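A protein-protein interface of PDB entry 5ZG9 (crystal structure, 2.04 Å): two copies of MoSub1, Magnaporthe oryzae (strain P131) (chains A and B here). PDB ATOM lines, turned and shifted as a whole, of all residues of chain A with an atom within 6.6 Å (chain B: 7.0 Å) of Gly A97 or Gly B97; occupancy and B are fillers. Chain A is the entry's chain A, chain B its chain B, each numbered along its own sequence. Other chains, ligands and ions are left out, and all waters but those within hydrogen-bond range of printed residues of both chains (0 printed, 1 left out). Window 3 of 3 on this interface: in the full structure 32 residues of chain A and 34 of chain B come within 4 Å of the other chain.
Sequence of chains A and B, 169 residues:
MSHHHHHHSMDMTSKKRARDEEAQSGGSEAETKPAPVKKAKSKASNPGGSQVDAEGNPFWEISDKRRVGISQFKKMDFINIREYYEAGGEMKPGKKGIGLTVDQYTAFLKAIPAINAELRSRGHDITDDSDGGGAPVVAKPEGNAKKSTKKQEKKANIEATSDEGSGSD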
ATOM      1  N   ILE A  81       0.127   3.994 -29.919  1.00  0.00           N
ATOM      2  CA  ILE A  81      -0.074   4.611 -31.226  1.00  0.00           C
ATOM      3  C   ILE A  81       1.250   5.294 -31.564  1.00  0.00           C
ATOM      4  O   ILE A  81       1.591   6.318 -30.958  1.00  0.00           O
ATOM      5  CB  ILE A  81      -1.218   5.662 -31.166  1.00  0.00           C
ATOM      6  CG1 ILE A  81      -2.473   5.033 -30.555  1.00  0.00           C
ATOM      7  CG2 ILE A  81      -1.513   6.258 -32.555  1.00  0.00           C
ATOM      8  CD1 ILE A  81      -3.612   6.007 -30.288  1.00  0.00           C
ATOM      9  N   ARG A  82       2.010   4.742 -32.508  1.00  0.00           N
ATOM     10  CA  ARG A  82       3.398   5.167 -32.626  1.00  0.00           C
ATOM     11  C   ARG A  82       3.953   5.088 -34.038  1.00  0.00           C
ATOM     12  O   ARG A  82       3.508   4.254 -34.839  1.00  0.00           O
ATOM     13  CB  ARG A  82       4.258   4.306 -31.699  1.00  0.00           C
ATOM     14  CG  ARG A  82       5.720   4.784 -31.550  1.00  0.00           C
ATOM     15  CD  ARG A  82       6.353   4.140 -30.316  1.00  0.00           C
ATOM     16  NE  ARG A  82       5.655   4.586 -29.119  1.00  0.00           N
ATOM     17  CZ  ARG A  82       5.903   5.747 -28.500  1.00  0.00           C
ATOM     18  NH1 ARG A  82       6.838   6.571 -28.963  1.00  0.00           N
ATOM     19  NH2 ARG A  82       5.212   6.087 -27.412  1.00  0.00           N
ATOM     20  N   GLU A  83       4.922   5.961 -34.318  1.00  0.00           N
ATOM     21  CA  GLU A  83       5.739   5.898 -35.523  1.00  0.00           C
ATOM     22  C   GLU A  83       6.752   4.764 -35.409  1.00  0.00           C
ATOM     23  O   GLU A  83       7.364   4.580 -34.356  1.00  0.00           O
ATOM     24  CB  GLU A  83       6.539   7.185 -35.684  1.00  0.00           C
ATOM     25  CG  GLU A  83       5.805   8.333 -36.308  1.00  0.00           C
ATOM     26  CD  GLU A  83       6.765   9.449 -36.686  1.00  0.00           C
ATOM     27  OE1 GLU A  83       8.000   9.228 -36.582  1.00  0.00           O
ATOM     28  OE2 GLU A  83       6.287  10.535 -37.091  1.00  0.00           O
ATOM     29  N   GLY A  94       9.481   4.181 -32.826  1.00  0.00           N
ATOM     30  CA  GLY A  94      10.133   5.473 -32.887  1.00  0.00           C
ATOM     31  C   GLY A  94       9.719   6.334 -31.709  1.00  0.00           C
ATOM     32  O   GLY A  94       8.953   5.897 -30.832  1.00  0.00           O
ATOM     33  N   LYS A  95      10.213   7.563 -31.665  1.00  0.00           N
ATOM     34  CA  LYS A  95       9.985   8.342 -30.454  1.00  0.00           C
ATOM     35  C   LYS A  95       8.710   9.184 -30.532  1.00  0.00           C
ATOM     36  O   LYS A  95       8.217   9.657 -29.515  1.00  0.00           O
ATOM     37  CB  LYS A  95      11.210   9.161 -30.071  1.00  0.00           C
ATOM     38  CG  LYS A  95      11.409  10.434 -30.839  1.00  0.00           C
ATOM     39  CD  LYS A  95      12.638  11.156 -30.288  1.00  0.00           C
ATOM     40  CE  LYS A  95      12.851  12.496 -30.972  1.00  0.00           C
ATOM     41  NZ  LYS A  95      14.221  13.029 -30.732  1.00  0.00           N
ATOM     42  N   LYS A  96       8.157   9.335 -31.735  1.00  0.00           N
ATOM     43  CA  LYS A  96       6.875  10.000 -31.883  1.00  0.00           C
ATOM     44  C   LYS A  96       5.743   8.993 -31.666  1.00  0.00           C
ATOM     45  O   LYS A  96       5.553   8.075 -32.477  1.00  0.00           O
ATOM     46  CB  LYS A  96       6.741  10.622 -33.276  1.00  0.00           C
ATOM     47  CG  LYS A  96       7.649  11.807 -33.548  1.00  0.00           C
ATOM     48  CD  LYS A  96       7.168  12.468 -34.832  1.00  0.00           C
ATOM     49  CE  LYS A  96       7.755  13.839 -35.066  1.00  0.00           C
ATOM     50  NZ  LYS A  96       7.145  14.445 -36.293  1.00  0.00           N
ATOM     51  N   GLY A  97       4.982   9.175 -30.587  1.00  0.00           N
ATOM     52  CA  GLY A  97       3.836   8.319 -30.332  1.00  0.00           C
ATOM     53  C   GLY A  97       3.424   8.415 -28.881  1.00  0.00           C
ATOM     54  O   GLY A  97       4.005   9.193 -28.114  1.00  0.00           O
ATOM     55  N   ILE A  98       2.442   7.619 -28.482  1.00  0.00           N
ATOM     56  CA  ILE A  98       2.025   7.654 -27.098  1.00  0.00           C
ATOM     57  C   ILE A  98       1.443   6.306 -26.715  1.00  0.00           C
ATOM     58  O   ILE A  98       0.863   5.605 -27.564  1.00  0.00           O
ATOM     59  CB  ILE A  98       1.010   8.790 -26.844  1.00  0.00           C
ATOM     60  CG1 ILE A  98       0.830   9.043 -25.334  1.00  0.00           C
ATOM     61  CG2 ILE A  98      -0.315   8.490 -27.518  1.00  0.00           C
ATOM     62  CD1 ILE A  98      -0.104  10.192 -25.040  1.00  0.00           C
ATOM     63  N   GLY A  99       1.628   5.938 -25.450  1.00  0.00           N
ATOM     64  CA  GLY A  99       1.111   4.679 -24.941  1.00  0.00           C
ATOM     65  C   GLY A  99      -0.021   4.928 -23.965  1.00  0.00           C
ATOM     66  O   GLY A  99       0.205   5.496 -22.892  1.00  0.00           O
ATOM     67  N   ASN B  80      -4.671  15.232 -32.388  1.00  0.00           N
ATOM     68  CA  ASN B  80      -3.530  15.008 -31.507  1.00  0.00           C
ATOM     69  C   ASN B  80      -3.949  14.336 -30.205  1.00  0.00           C
ATOM     70  O   ASN B  80      -4.881  14.789 -29.526  1.00  0.00           O
ATOM     71  CB  ASN B  80      -2.848  16.338 -31.157  1.00  0.00           C
ATOM     72  CG  ASN B  80      -1.798  16.740 -32.170  1.00  0.00           C
ATOM     73  OD1 ASN B  80      -0.607  16.388 -32.040  1.00  0.00           O
ATOM     74  ND2 ASN B  80      -2.224  17.476 -33.196  1.00  0.00           N
ATOM     75  N   ILE B  81      -3.246  13.267 -29.859  1.00  0.00           N
ATOM     76  CA  ILE B  81      -3.430  12.553 -28.594  1.00  0.00           C
ATOM     77  C   ILE B  81      -2.105  12.765 -27.888  1.00  0.00           C
ATOM     78  O   ILE B  81      -1.073  12.234 -28.330  1.00  0.00           O
ATOM     79  CB  ILE B  81      -3.598  11.056 -28.856  1.00  0.00           C
ATOM     80  CG1 ILE B  81      -4.726  10.841 -29.879  1.00  0.00           C
ATOM     81  CG2 ILE B  81      -3.876  10.307 -27.554  1.00  0.00           C
ATOM     82  CD1 ILE B  81      -4.710   9.477 -30.556  1.00  0.00           C
ATOM     83  N   ARG B  82      -2.099  13.547 -26.813  1.00  0.00           N
ATOM     84  CA  ARG B  82      -0.836  14.143 -26.379  1.00  0.00           C
ATOM     85  C   ARG B  82      -0.855  14.479 -24.902  1.00  0.00           C
ATOM     86  O   ARG B  82      -1.906  14.823 -24.342  1.00  0.00           O
ATOM     87  CB  ARG B  82      -0.577  15.415 -27.218  1.00  0.00           C
ATOM     88  CG  ARG B  82       0.744  16.138 -26.931  1.00  0.00           C
ATOM     89  CD  ARG B  82       1.066  17.181 -28.010  1.00  0.00           C
ATOM     90  NE  ARG B  82       1.194  16.551 -29.328  1.00  0.00           N
ATOM     91  CZ  ARG B  82       2.295  15.912 -29.746  1.00  0.00           C
ATOM     92  NH1 ARG B  82       3.370  15.827 -28.949  1.00  0.00           N
ATOM     93  NH2 ARG B  82       2.332  15.349 -30.958  1.00  0.00           N
ATOM     94  N   GLU B  83       0.317  14.378 -24.285  1.00  0.00           N
ATOM     95  CA  GLU B  83       0.526  14.761 -22.893  1.00  0.00           C
ATOM     96  C   GLU B  83       0.647  16.296 -22.773  1.00  0.00           C
ATOM     97  O   GLU B  83       1.305  16.938 -23.607  1.00  0.00           O
ATOM     98  CB  GLU B  83       1.821  14.103 -22.418  1.00  0.00           C
ATOM     99  CG  GLU B  83       1.882  13.738 -20.947  1.00  0.00           C
ATOM    100  CD  GLU B  83       3.105  12.887 -20.626  1.00  0.00           C
ATOM    101  OE1 GLU B  83       2.988  11.639 -20.608  1.00  0.00           O
ATOM    102  OE2 GLU B  83       4.187  13.472 -20.401  1.00  0.00           O
ATOM    103  N   GLY B  94       2.863  18.966 -24.837  1.00  0.00           N
ATOM    104  CA  GLY B  94       4.189  18.432 -24.574  1.00  0.00           C
ATOM    105  C   GLY B  94       4.778  17.590 -25.695  1.00  0.00           C
ATOM    106  O   GLY B  94       4.177  17.463 -26.769  1.00  0.00           O
ATOM    107  N   LYS B  95       5.953  17.013 -25.445  1.00  0.00           N
ATOM    108  CA  LYS B  95       6.688  16.272 -26.476  1.00  0.00           C
ATOM    109  C   LYS B  95       6.152  14.868 -26.728  1.00  0.00           C
ATOM    110  O   LYS B  95       6.254  14.361 -27.843  1.00  0.00           O
ATOM    111  CB  LYS B  95       8.178  16.198 -26.140  1.00  0.00           C
ATOM    112  N   LYS B  96       5.575  14.256 -25.699  1.00  0.00           N
ATOM    113  CA  LYS B  96       5.031  12.904 -25.801  1.00  0.00           C
ATOM    114  C   LYS B  96       3.621  12.924 -26.363  1.00  0.00           C
ATOM    115  O   LYS B  96       2.706  13.486 -25.755  1.00  0.00           O
ATOM    116  CB  LYS B  96       4.997  12.223 -24.424  1.00  0.00           C
ATOM    117  CG  LYS B  96       6.352  12.086 -23.776  1.00  0.00           C
ATOM    118  CD  LYS B  96       6.245  11.455 -22.394  1.00  0.00           C
ATOM    119  CE  LYS B  96       5.637  10.069 -22.441  1.00  0.00           C
ATOM    120  NZ  LYS B  96       5.925   9.338 -21.161  1.00  0.00           N
ATOM    121  N   GLY B  97       3.438  12.293 -27.515  1.00  0.00           N
ATOM    122  CA  GLY B  97       2.121  12.212 -28.122  1.00  0.00           C
ATOM    123  C   GLY B  97       2.292  12.050 -29.610  1.00  0.00           C
ATOM    124  O   GLY B  97       3.429  11.888 -30.099  1.00  0.00           O
ATOM    125  N   ILE B  98       1.178  12.110 -30.331  1.00  0.00           N
ATOM    126  CA  ILE B  98       1.210  11.964 -31.773  1.00  0.00           C
ATOM    127  C   ILE B  98       0.029  12.704 -32.420  1.00  0.00           C
ATOM    128  O   ILE B  98      -1.072  12.769 -31.844  1.00  0.00           O
ATOM    129  CB  ILE B  98       1.206  10.465 -32.150  1.00  0.00           C
ATOM    130  CG1 ILE B  98       1.567  10.271 -33.618  1.00  0.00           C
ATOM    131  CG2 ILE B  98      -0.170   9.817 -31.802  1.00  0.00           C
ATOM    132  CD1 ILE B  98       1.899   8.805 -33.949  1.00  0.00           C
ATOM    133  N   GLY B  99       0.264  13.271 -33.607  1.00  0.00           N
ATOM    134  CA  GLY B  99      -0.779  13.959 -34.357  1.00  0.00           C
ATOM    135  C   GLY B  99      -1.162  13.140 -35.579  1.00  0.00           C
ATOM    136  O   GLY B  99      -0.332  12.911 -36.468  1.00  0.00           O
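O of Gly B97 is in hydrogen-bond range of N of Gly A97, 3.2 Å away.
O of Ile A81 lies within hydrogen-bond range of N of Ile A98. The backbone carbonyl oxygen (O) of Gly A97 lies close to the guanidinium group (NH2) of Arg A82, 3.4 Å away. The backbone NH (N) of Ile B81 sits at hydrogen-bond distance from the backbone carbonyl oxygen (O) of Ile B98, 3.0 Å away.
Among the printed residues, pairs that only touch across the chains: Ile A81 with Ile B81 (3.6 Å), Ile A98 with Gly B97 (3.8 Å), Gly A97 with Ile B98 (3.9 Å), Ile A81 with Ile B98 (3.9 Å) and Ile A98 with Ile B81 (3.9 Å).
Of chain A, only Gly A97 and Ile A98 come within 4 Å of Gly B97. Of the printed residues of chain B, Ile A98 touches Ile B81 (3.9 Å) and Gly B97 (3.8 Å). Of the printed residues of chain A, Ile B81 touches Ile A81 (3.6 Å) and Ile A98 (3.9 Å). Of the printed residues of chain B, Ile A81 touches Ile B81 and Ile B98. Of the printed residues of chain A, Ile B98 touches Ile A81 (3.9 Å) and Gly A97 (3.9 Å). Asn B80 touches none of the printed residues of chain A. The nearest residue of chain B that does not touch Gly A97 is Lys B96 (4.1 Å). The nearest printed residue of chain A that does not touch Ile B81 is Gly A97 (5.9 Å).
Of the 9 printed residues of chain A, 3 touch a printed residue of chain B. Hydrophobic or aromatic side chains of chain A that line the printed part of chain B: Ile A81 and Ile A98. Printed residues of chain B that touch a printed residue of chain A: Ile B81, Gly B97 and Ile B98. Among the printed residues, 6 pairs touch across the chains. Among the printed residues, no Asp or Glu carboxylate lies within 4 Å of a Lys or Arg side-chain nitrogen of the other chain.
Ile B81 touches its own counterpart, Ile A81. Ile A81 touches Ile B98, and with the chains exchanged Ile A98 touches Ile B81. Gly B97 touches its own counterpart, Gly A97. Gly A97 touches Ile B98, and with the chains exchanged Ile A98 touches Gly B97. Of the 6 pairs that touch across the chains among the printed residues, 6 have their exchanged pair printed and touching as well.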
